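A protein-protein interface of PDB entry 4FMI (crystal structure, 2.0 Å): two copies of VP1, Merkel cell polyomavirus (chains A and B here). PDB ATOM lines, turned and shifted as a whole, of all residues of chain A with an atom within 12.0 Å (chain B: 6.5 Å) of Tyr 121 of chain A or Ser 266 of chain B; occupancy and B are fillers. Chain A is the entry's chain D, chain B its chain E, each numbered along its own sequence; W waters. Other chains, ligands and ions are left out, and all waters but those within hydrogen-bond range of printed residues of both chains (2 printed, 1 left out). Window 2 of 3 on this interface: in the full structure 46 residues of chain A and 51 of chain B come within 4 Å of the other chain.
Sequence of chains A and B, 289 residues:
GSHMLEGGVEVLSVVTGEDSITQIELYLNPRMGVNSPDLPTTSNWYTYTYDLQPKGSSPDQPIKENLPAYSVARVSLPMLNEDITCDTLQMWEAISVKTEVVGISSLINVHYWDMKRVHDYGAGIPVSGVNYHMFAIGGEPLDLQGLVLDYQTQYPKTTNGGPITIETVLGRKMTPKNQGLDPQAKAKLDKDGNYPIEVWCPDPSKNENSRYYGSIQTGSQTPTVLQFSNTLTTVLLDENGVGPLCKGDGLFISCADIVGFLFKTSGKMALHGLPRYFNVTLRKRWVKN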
ATOM      1  N   VAL A 110     -13.070  10.772 -17.370  1.00  0.00           N
ATOM      2  CA  VAL A 110     -14.191   9.833 -17.252  1.00  0.00           C
ATOM      3  C   VAL A 110     -14.765   9.841 -15.831  1.00  0.00           C
ATOM      4  O   VAL A 110     -15.335   8.854 -15.376  1.00  0.00           O
ATOM      5  CB  VAL A 110     -13.804   8.379 -17.716  1.00  0.00           C
ATOM      6  CG1 VAL A 110     -13.519   8.365 -19.217  1.00  0.00           C
ATOM      7  CG2 VAL A 110     -12.609   7.844 -16.946  1.00  0.00           C
ATOM      8  N   HIS A 111     -14.626  10.978 -15.151  1.00  0.00           N
ATOM      9  CA  HIS A 111     -15.002  11.103 -13.739  1.00  0.00           C
ATOM     10  C   HIS A 111     -15.653  12.463 -13.462  1.00  0.00           C
ATOM     11  O   HIS A 111     -15.452  13.071 -12.409  1.00  0.00           O
ATOM     12  CB  HIS A 111     -13.788  10.880 -12.836  1.00  0.00           C
ATOM     13  CG  HIS A 111     -12.661  11.815 -13.125  1.00  0.00           C
ATOM     14  ND1 HIS A 111     -12.566  13.063 -12.549  1.00  0.00           N
ATOM     15  CD2 HIS A 111     -11.607  11.706 -13.968  1.00  0.00           C
ATOM     16  CE1 HIS A 111     -11.488  13.674 -13.006  1.00  0.00           C
ATOM     17  NE2 HIS A 111     -10.886  12.870 -13.866  1.00  0.00           N
ATOM     18  N   TYR A 112     -16.444  12.932 -14.425  1.00  0.00           N
ATOM     19  CA  TYR A 112     -17.316  14.059 -14.189  1.00  0.00           C
ATOM     20  C   TYR A 112     -18.280  13.629 -13.080  1.00  0.00           C
ATOM     21  O   TYR A 112     -18.755  12.481 -13.074  1.00  0.00           O
ATOM     22  CB  TYR A 112     -18.049  14.436 -15.473  1.00  0.00           C
ATOM     23  CG  TYR A 112     -19.229  15.346 -15.268  1.00  0.00           C
ATOM     24  CD1 TYR A 112     -19.072  16.615 -14.705  1.00  0.00           C
ATOM     25  CD2 TYR A 112     -20.503  14.947 -15.660  1.00  0.00           C
ATOM     26  CE1 TYR A 112     -20.156  17.447 -14.518  1.00  0.00           C
ATOM     27  CE2 TYR A 112     -21.589  15.778 -15.487  1.00  0.00           C
ATOM     28  CZ  TYR A 112     -21.411  17.024 -14.910  1.00  0.00           C
ATOM     29  OH  TYR A 112     -22.500  17.847 -14.724  1.00  0.00           O
ATOM     30  N   TRP A 113     -18.550  14.535 -12.138  1.00  0.00           N
ATOM     31  CA  TRP A 113     -19.242  14.160 -10.891  1.00  0.00           C
ATOM     32  C   TRP A 113     -20.611  13.559 -11.168  1.00  0.00           C
ATOM     33  O   TRP A 113     -21.044  12.656 -10.470  1.00  0.00           O
ATOM     34  CB  TRP A 113     -19.293  15.316  -9.870  1.00  0.00           C
ATOM     35  CG  TRP A 113     -20.302  16.414 -10.161  1.00  0.00           C
ATOM     36  CD1 TRP A 113     -20.050  17.639 -10.723  1.00  0.00           C
ATOM     37  CD2 TRP A 113     -21.715  16.375  -9.906  1.00  0.00           C
ATOM     38  NE1 TRP A 113     -21.218  18.362 -10.829  1.00  0.00           N
ATOM     39  CE2 TRP A 113     -22.254  17.615 -10.331  1.00  0.00           C
ATOM     40  CE3 TRP A 113     -22.577  15.417  -9.352  1.00  0.00           C
ATOM     41  CZ2 TRP A 113     -23.617  17.917 -10.229  1.00  0.00           C
ATOM     42  CZ3 TRP A 113     -23.938  15.722  -9.246  1.00  0.00           C
ATOM     43  CH2 TRP A 113     -24.443  16.964  -9.690  1.00  0.00           C
ATOM     44  N   MET A 115     -21.518  12.011 -14.112  1.00  0.00           N
ATOM     45  CA  MET A 115     -21.384  11.235 -15.352  1.00  0.00           C
ATOM     46  C   MET A 115     -22.106   9.900 -15.231  1.00  0.00           C
ATOM     47  O   MET A 115     -21.955   9.202 -14.229  1.00  0.00           O
ATOM     48  CB  MET A 115     -19.909  10.996 -15.670  1.00  0.00           C
ATOM     49  CG  MET A 115     -19.539  11.201 -17.131  1.00  0.00           C
ATOM     50  SD  MET A 115     -17.757  11.081 -17.331  1.00  0.00           S
ATOM     51  CE  MET A 115     -17.519  12.218 -18.701  1.00  0.00           C
ATOM     52  N   LYS A 116     -22.903   9.549 -16.242  1.00  0.00           N
ATOM     53  CA  LYS A 116     -23.505   8.222 -16.301  1.00  0.00           C
ATOM     54  C   LYS A 116     -22.414   7.153 -16.454  1.00  0.00           C
ATOM     55  O   LYS A 116     -21.498   7.308 -17.253  1.00  0.00           O
ATOM     56  CB  LYS A 116     -24.515   8.131 -17.445  1.00  0.00           C
ATOM     57  CG  LYS A 116     -25.171   6.760 -17.604  1.00  0.00           C
ATOM     58  CD  LYS A 116     -26.239   6.790 -18.695  1.00  0.00           C
ATOM     59  CE  LYS A 116     -26.793   5.398 -18.990  1.00  0.00           C
ATOM     60  NZ  LYS A 116     -27.636   4.873 -17.893  1.00  0.00           N
ATOM     61  N   ARG A 117     -22.519   6.081 -15.674  1.00  0.00           N
ATOM     62  CA  ARG A 117     -21.519   5.000 -15.679  1.00  0.00           C
ATOM     63  C   ARG A 117     -21.734   4.020 -16.828  1.00  0.00           C
ATOM     64  O   ARG A 117     -22.872   3.796 -17.265  1.00  0.00           O
ATOM     65  CB  ARG A 117     -21.566   4.233 -14.355  1.00  0.00           C
ATOM     66  CG  ARG A 117     -21.006   4.978 -13.144  1.00  0.00           C
ATOM     67  CD  ARG A 117     -21.337   4.192 -11.881  1.00  0.00           C
ATOM     68  NE  ARG A 117     -21.062   4.906 -10.634  1.00  0.00           N
ATOM     69  CZ  ARG A 117     -19.930   4.818  -9.935  1.00  0.00           C
ATOM     70  NH1 ARG A 117     -18.916   4.075 -10.364  1.00  0.00           N
ATOM     71  NH2 ARG A 117     -19.806   5.487  -8.798  1.00  0.00           N
ATOM     72  N   VAL A 118     -20.643   3.433 -17.313  1.00  0.00           N
ATOM     73  CA  VAL A 118     -20.729   2.385 -18.331  1.00  0.00           C
ATOM     74  C   VAL A 118     -21.416   1.132 -17.767  1.00  0.00           C
ATOM     75  O   VAL A 118     -22.128   0.425 -18.489  1.00  0.00           O
ATOM     76  CB  VAL A 118     -19.344   2.041 -18.932  1.00  0.00           C
ATOM     77  CG1 VAL A 118     -18.669   3.300 -19.471  1.00  0.00           C
ATOM     78  CG2 VAL A 118     -18.463   1.367 -17.906  1.00  0.00           C
ATOM     79  N   HIS A 119     -21.196   0.881 -16.476  1.00  0.00           N
ATOM     80  CA  HIS A 119     -21.864  -0.192 -15.723  1.00  0.00           C
ATOM     81  C   HIS A 119     -21.662   0.102 -14.239  1.00  0.00           C
ATOM     82  O   HIS A 119     -20.951   1.058 -13.887  1.00  0.00           O
ATOM     83  CB  HIS A 119     -21.318  -1.594 -16.079  1.00  0.00           C
ATOM     84  CG  HIS A 119     -19.827  -1.714 -15.977  1.00  0.00           C
ATOM     85  ND1 HIS A 119     -19.029  -2.008 -17.062  1.00  0.00           N
ATOM     86  CD2 HIS A 119     -18.989  -1.580 -14.920  1.00  0.00           C
ATOM     87  CE1 HIS A 119     -17.765  -2.050 -16.678  1.00  0.00           C
ATOM     88  NE2 HIS A 119     -17.713  -1.790 -15.384  1.00  0.00           N
ATOM     89  N   ASP A 120     -22.276  -0.714 -13.374  1.00  0.00           N
ATOM     90  CA  ASP A 120     -22.130  -0.560 -11.934  1.00  0.00           C
ATOM     91  C   ASP A 120     -20.667  -0.499 -11.514  1.00  0.00           C
ATOM     92  O   ASP A 120     -19.865  -1.360 -11.886  1.00  0.00           O
ATOM     93  CB  ASP A 120     -22.846  -1.695 -11.175  1.00  0.00           C
ATOM     94  CG  ASP A 120     -24.348  -1.487 -11.084  1.00  0.00           C
ATOM     95  OD1 ASP A 120     -24.824  -0.367 -11.365  1.00  0.00           O
ATOM     96  OD2 ASP A 120     -25.054  -2.453 -10.719  1.00  0.00           O
ATOM     97  N   TYR A 121     -20.337   0.530 -10.738  1.00  0.00           N
ATOM     98  CA  TYR A 121     -18.989   0.732 -10.175  1.00  0.00           C
ATOM     99  C   TYR A 121     -17.956   1.159 -11.215  1.00  0.00           C
ATOM    100  O   TYR A 121     -16.764   1.320 -10.897  1.00  0.00           O
ATOM    101  CB  TYR A 121     -18.525  -0.497  -9.387  1.00  0.00           C
ATOM    102  CG  TYR A 121     -19.484  -0.867  -8.270  1.00  0.00           C
ATOM    103  CD1 TYR A 121     -20.376  -1.931  -8.411  1.00  0.00           C
ATOM    104  CD2 TYR A 121     -19.511  -0.135  -7.078  1.00  0.00           C
ATOM    105  CE1 TYR A 121     -21.271  -2.265  -7.380  1.00  0.00           C
ATOM    106  CE2 TYR A 121     -20.389  -0.458  -6.050  1.00  0.00           C
ATOM    107  CZ  TYR A 121     -21.267  -1.519  -6.206  1.00  0.00           C
ATOM    108  OH  TYR A 121     -22.136  -1.828  -5.181  1.00  0.00           O
ATOM    109  N   GLY A 122     -18.428   1.377 -12.440  1.00  0.00           N
ATOM    110  CA  GLY A 122     -17.548   1.710 -13.559  1.00  0.00           C
ATOM    111  C   GLY A 122     -17.220   3.183 -13.667  1.00  0.00           C
ATOM    112  O   GLY A 122     -17.743   4.017 -12.917  1.00  0.00           O
ATOM    113  N   ALA A 123     -16.342   3.497 -14.615  1.00  0.00           N
ATOM    114  CA  ALA A 123     -16.036   4.868 -14.965  1.00  0.00           C
ATOM    115  C   ALA A 123     -17.219   5.478 -15.717  1.00  0.00           C
ATOM    116  O   ALA A 123     -18.129   4.763 -16.154  1.00  0.00           O
ATOM    117  CB  ALA A 123     -14.766   4.930 -15.811  1.00  0.00           C
ATOM    118  N   GLY A 124     -17.213   6.798 -15.845  1.00  0.00           N
ATOM    119  CA  GLY A 124     -18.204   7.484 -16.680  1.00  0.00           C
ATOM    120  C   GLY A 124     -18.068   7.106 -18.145  1.00  0.00           C
ATOM    121  O   GLY A 124     -16.992   6.727 -18.605  1.00  0.00           O
ATOM    122  N   ILE A 125     -19.186   7.155 -18.863  1.00  0.00           N
ATOM    123  CA  ILE A 125     -19.183   7.063 -20.316  1.00  0.00           C
ATOM    124  C   ILE A 125     -18.469   8.314 -20.832  1.00  0.00           C
ATOM    125  O   ILE A 125     -18.878   9.419 -20.514  1.00  0.00           O
ATOM    126  CB  ILE A 125     -20.632   7.032 -20.878  1.00  0.00           C
ATOM    127  CG1 ILE A 125     -21.400   5.818 -20.325  1.00  0.00           C
ATOM    128  CG2 ILE A 125     -20.622   7.081 -22.400  1.00  0.00           C
ATOM    129  CD1 ILE A 125     -22.922   5.888 -20.530  1.00  0.00           C
ATOM    130  N   THR A 265     -26.057  11.201 -15.221  1.00  0.00           N
ATOM    131  CA  THR A 265     -26.626  10.106 -14.408  1.00  0.00           C
ATOM    132  C   THR A 265     -28.116   9.820 -14.686  1.00  0.00           C
ATOM    133  O   THR A 265     -28.496   8.675 -14.953  1.00  0.00           O
ATOM    134  CB  THR A 265     -26.408  10.362 -12.898  1.00  0.00           C
ATOM    135  OG1 THR A 265     -25.031  10.683 -12.667  1.00  0.00           O
ATOM    136  CG2 THR A 265     -26.778   9.127 -12.078  1.00  0.00           C
ATOM    137  N   ASP B  51      -9.112   3.577  -9.272  1.00  0.00           N
ATOM    138  CA  ASP B  51     -10.410   3.336  -9.883  1.00  0.00           C
ATOM    139  C   ASP B  51     -11.095   4.654 -10.215  1.00  0.00           C
ATOM    140  O   ASP B  51     -11.274   5.519  -9.351  1.00  0.00           O
ATOM    141  CB  ASP B  51     -11.273   2.435  -8.993  1.00  0.00           C
ATOM    142  CG  ASP B  51     -10.599   1.094  -8.684  1.00  0.00           C
ATOM    143  OD1 ASP B  51     -10.593   0.696  -7.503  1.00  0.00           O
ATOM    144  OD2 ASP B  51     -10.067   0.442  -9.612  1.00  0.00           O
ATOM    145  N   LEU B  52     -11.431   4.815 -11.490  1.00  0.00           N
ATOM    146  CA  LEU B  52     -12.085   6.025 -11.968  1.00  0.00           C
ATOM    147  C   LEU B  52     -13.588   5.875 -11.845  1.00  0.00           C
ATOM    148  O   LEU B  52     -14.169   4.941 -12.398  1.00  0.00           O
ATOM    149  CB  LEU B  52     -11.700   6.314 -13.418  1.00  0.00           C
ATOM    150  CG  LEU B  52     -10.256   6.770 -13.624  1.00  0.00           C
ATOM    151  CD1 LEU B  52      -9.781   6.451 -15.036  1.00  0.00           C
ATOM    152  CD2 LEU B  52     -10.079   8.262 -13.315  1.00  0.00           C
ATOM    153  N   GLN B  53     -14.206   6.802 -11.118  1.00  0.00           N
ATOM    154  CA  GLN B  53     -15.641   6.788 -10.881  1.00  0.00           C
ATOM    155  C   GLN B  53     -16.149   8.212 -10.805  1.00  0.00           C
ATOM    156  O   GLN B  53     -15.467   9.080 -10.263  1.00  0.00           O
ATOM    157  CB  GLN B  53     -15.978   6.111  -9.542  1.00  0.00           C
ATOM    158  CG  GLN B  53     -15.586   4.638  -9.392  1.00  0.00           C
ATOM    159  CD  GLN B  53     -16.012   4.087  -8.039  1.00  0.00           C
ATOM    160  OE1 GLN B  53     -17.172   3.744  -7.843  1.00  0.00           O
ATOM    161  NE2 GLN B  53     -15.078   4.030  -7.093  1.00  0.00           N
ATOM    162  N   ASP B 114      -8.121 -10.629 -11.739  1.00  0.00           N
ATOM    163  CA  ASP B 114      -9.328  -9.900 -11.354  1.00  0.00           C
ATOM    164  C   ASP B 114      -9.938  -9.181 -12.556  1.00  0.00           C
ATOM    165  O   ASP B 114     -10.471  -8.064 -12.434  1.00  0.00           O
ATOM    166  CB  ASP B 114      -9.032  -8.895 -10.218  1.00  0.00           C
ATOM    167  CG  ASP B 114     -10.277  -8.542  -9.404  1.00  0.00           C
ATOM    168  OD1 ASP B 114     -11.215  -9.351  -9.378  1.00  0.00           O
ATOM    169  OD2 ASP B 114     -10.329  -7.453  -8.799  1.00  0.00           O
ATOM    170  N   LYS B 116     -12.670  -8.499 -15.288  1.00  0.00           N
ATOM    171  CA  LYS B 116     -14.081  -8.700 -15.585  1.00  0.00           C
ATOM    172  C   LYS B 116     -14.208  -9.574 -16.832  1.00  0.00           C
ATOM    173  O   LYS B 116     -13.544  -9.334 -17.842  1.00  0.00           O
ATOM    174  CB  LYS B 116     -14.787  -7.365 -15.792  1.00  0.00           C
ATOM    175  CG  LYS B 116     -16.291  -7.472 -16.041  1.00  0.00           C
ATOM    176  CD  LYS B 116     -16.959  -6.106 -15.881  1.00  0.00           C
ATOM    177  CE  LYS B 116     -18.433  -6.136 -16.284  1.00  0.00           C
ATOM    178  NZ  LYS B 116     -19.241  -7.083 -15.449  1.00  0.00           N
ATOM    179  N   LYS B 264     -12.100  -4.523 -14.130  1.00  0.00           N
ATOM    180  CA  LYS B 264     -12.017  -5.387 -12.952  1.00  0.00           C
ATOM    181  C   LYS B 264     -13.346  -6.079 -12.649  1.00  0.00           C
ATOM    182  O   LYS B 264     -14.418  -5.597 -13.051  1.00  0.00           O
ATOM    183  CB  LYS B 264     -11.511  -4.591 -11.733  1.00  0.00           C
ATOM    184  CG  LYS B 264     -10.136  -3.946 -11.935  1.00  0.00           C
ATOM    185  CD  LYS B 264      -9.797  -2.938 -10.812  1.00  0.00           C
ATOM    186  CE  LYS B 264      -8.439  -2.259 -11.030  1.00  0.00           C
ATOM    187  NZ  LYS B 264      -8.004  -1.417  -9.854  1.00  0.00           N
ATOM    188  N   THR B 265     -13.263  -7.219 -11.955  1.00  0.00           N
ATOM    189  CA  THR B 265     -14.425  -8.072 -11.632  1.00  0.00           C
ATOM    190  C   THR B 265     -15.616  -7.285 -11.070  1.00  0.00           C
ATOM    191  O   THR B 265     -16.763  -7.473 -11.504  1.00  0.00           O
ATOM    192  CB  THR B 265     -14.024  -9.203 -10.626  1.00  0.00           C
ATOM    193  OG1 THR B 265     -12.952  -9.978 -11.181  1.00  0.00           O
ATOM    194  CG2 THR B 265     -15.204 -10.141 -10.314  1.00  0.00           C
ATOM    195  N   SER B 266     -15.324  -6.403 -10.116  1.00  0.00           N
ATOM    196  CA  SER B 266     -16.342  -5.639  -9.376  1.00  0.00           C
ATOM    197  C   SER B 266     -17.114  -4.638 -10.233  1.00  0.00           C
ATOM    198  O   SER B 266     -18.194  -4.191  -9.849  1.00  0.00           O
ATOM    199  CB  SER B 266     -15.658  -4.851  -8.261  1.00  0.00           C
ATOM    200  OG  SER B 266     -14.699  -3.973  -8.839  1.00  0.00           O
ATOM    201  N   GLY B 267     -16.542  -4.271 -11.376  1.00  0.00           N
ATOM    202  CA  GLY B 267     -17.092  -3.215 -12.233  1.00  0.00           C
ATOM    203  C   GLY B 267     -16.137  -2.045 -12.340  1.00  0.00           C
ATOM    204  O   GLY B 267     -16.202  -1.268 -13.289  1.00  0.00           O
ATOM    205  N   LYS B 268     -15.221  -1.940 -11.379  1.00  0.00           N
ATOM    206  CA  LYS B 268     -14.232  -0.874 -11.386  1.00  0.00           C
ATOM    207  C   LYS B 268     -13.288  -0.934 -12.582  1.00  0.00           C
ATOM    208  O   LYS B 268     -13.070  -2.001 -13.192  1.00  0.00           O
ATOM    209  CB  LYS B 268     -13.510  -0.762 -10.039  1.00  0.00           C
ATOM    210  CG  LYS B 268     -14.505  -0.324  -8.957  1.00  0.00           C
ATOM    211  CD  LYS B 268     -13.928  -0.208  -7.588  1.00  0.00           C
ATOM    212  CE  LYS B 268     -14.945   0.497  -6.677  1.00  0.00           C
ATOM    213  NZ  LYS B 268     -14.459   0.555  -5.291  1.00  0.00           N
ATOM    214  N   MET B 269     -12.780   0.246 -12.925  1.00  0.00           N
ATOM    215  CA  MET B 269     -12.024   0.470 -14.141  1.00  0.00           C
ATOM    216  C   MET B 269     -10.893   1.421 -13.851  1.00  0.00           C
ATOM    217  O   MET B 269     -11.112   2.511 -13.292  1.00  0.00           O
ATOM    218  CB  MET B 269     -12.928   1.104 -15.184  1.00  0.00           C
ATOM    219  CG  MET B 269     -13.822   0.120 -15.874  1.00  0.00           C
ATOM    220  SD  MET B 269     -15.270   0.907 -16.572  1.00  0.00           S
ATOM    221  CE  MET B 269     -14.587   1.691 -18.038  1.00  0.00           C
HETATM  222  O   HOH W   1     -14.118   2.437 -11.538  1.00  0.00           O
HETATM  223  O   HOH W   2     -18.110   6.709  -6.827  1.00  0.00           O
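Tyr 121 of chain A touches just these residues of chain B: Gln 53, Ser 266, Gly 267 and Lys 268.
No residue of chain A comes within 4 Å of Lys 264 of chain B.
Printed residues of chain A within 4 Å of Met 269 of chain B: Val 118, His 119, Gly 122 and Ala 123.
Of the printed residues of chain B, His 119 of chain A touches Gly 267 (2.6 Å) and Met 269 (3.8 Å).
Printed residues of chain B within 4 Å of His 111 of chain A: Leu 52 (3.8 Å) and Gln 53 (3.6 Å).
Printed residues of chain B within 4 Å of Arg 117 of chain A: Gln 53 (3.1 Å).
Printed residues of chain B within 4 Å of Val 118 of chain A: Met 269 (3.5 Å).
Lys 116 of chain B touches none of the printed residues of chain A.
The nearest residue of chain B that does not touch Tyr 121 of chain A is Met 269 of chain B (4.6 Å).
The nearest residue of chain A that does not touch Ser 266 of chain B is His 119 of chain A (5.8 Å).
N of Gly 124 of chain A lies within hydrogen-bond range of O of Val 110 of chain A.
O of Gly 122 of chain A lies within hydrogen-bond range of NH1 of Arg 117 of chain A.
N of Val 118 of chain A lies within hydrogen-bond range of O of Ala 123 of chain A (3.1 Å).
The backbone carbonyl oxygen of Met 269 of chain B sits at hydrogen-bond distance from the backbone NH of Leu 52 of chain B, at 2.9 Å.
The side-chain hydroxyl (OG) of Ser 266 of chain B is in hydrogen-bond range of the backbone NH (N) of Lys 268 of chain B (3.3 Å).
Leu 52 of chain B touches Val 110 of chain A.
CD2 of His 111 of chain A touches CD2 of Leu 52 of chain B (3.8 Å).
Val 118 of chain A touches Met 269 of chain B (CG2 to SD, 3.5 Å).
NE2 of His 119 of chain A touches SD of Met 269 of chain B, at 3.8 Å.
O of Ser 266 of chain B touches O of Asp 120 of chain A, at 3.9 Å.
Gly 267 of chain B touches Asp 120 of chain A (CA to O, 3.4 Å).
CD1 of Tyr 121 of chain A touches O of Ser 266 of chain B, 3.5 Å away.
Tyr 121 of chain A touches Lys 268 of chain B.
Gly 267 of chain B touches Gly 122 of chain A.
Met 269 of chain B touches Gly 122 of chain A (SD to CA, 3.9 Å).
Positions printed for both chains: 116 and 265.
Of the 18 pairs that touch across the chains among the printed residues, none has its exchanged pair printed and touching as well.
Of the 11 printed residues of chain B, 6 touch a printed residue of chain A.
Hydrophobic or aromatic side chains of chain B that line the printed part of chain A: Leu 52 and Met 269.
Along chain B the printed residues that touch a printed residue of chain A span positions 52 to 269.
Among the printed residues, 18 pairs touch across the chains.
Water W1 lies within hydrogen-bond range of O of Leu 52 of chain B (2.6 Å), N of Met 269 of chain B (2.9 Å) and O of Tyr 121 of chain A (2.9 Å).
Water W2 lies within hydrogen-bond range of the guanidinium group (NH2) of Arg 117 of chain A (2.9 Å) and the side-chain amide oxygen (OE1) of Gln 53 of chain B (3.3 Å).
NH1 of Arg 117 of chain A sits at hydrogen-bond distance from OE1 of Gln 53 of chain B (3.1 Å).
NE2 of His 119 of chain A is in hydrogen-bond range of O of Gly 267 of chain B (2.6 Å).
The backbone NH of Ala 123 of chain A lies close to the backbone carbonyl oxygen of Leu 52 of chain B, at 3.4 Å.
The side-chain sulfur (SD) of Met 269 of chain B lies within hydrogen-bond range of the backbone NH (N) of Ala 123 of chain A (3.4 Å).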
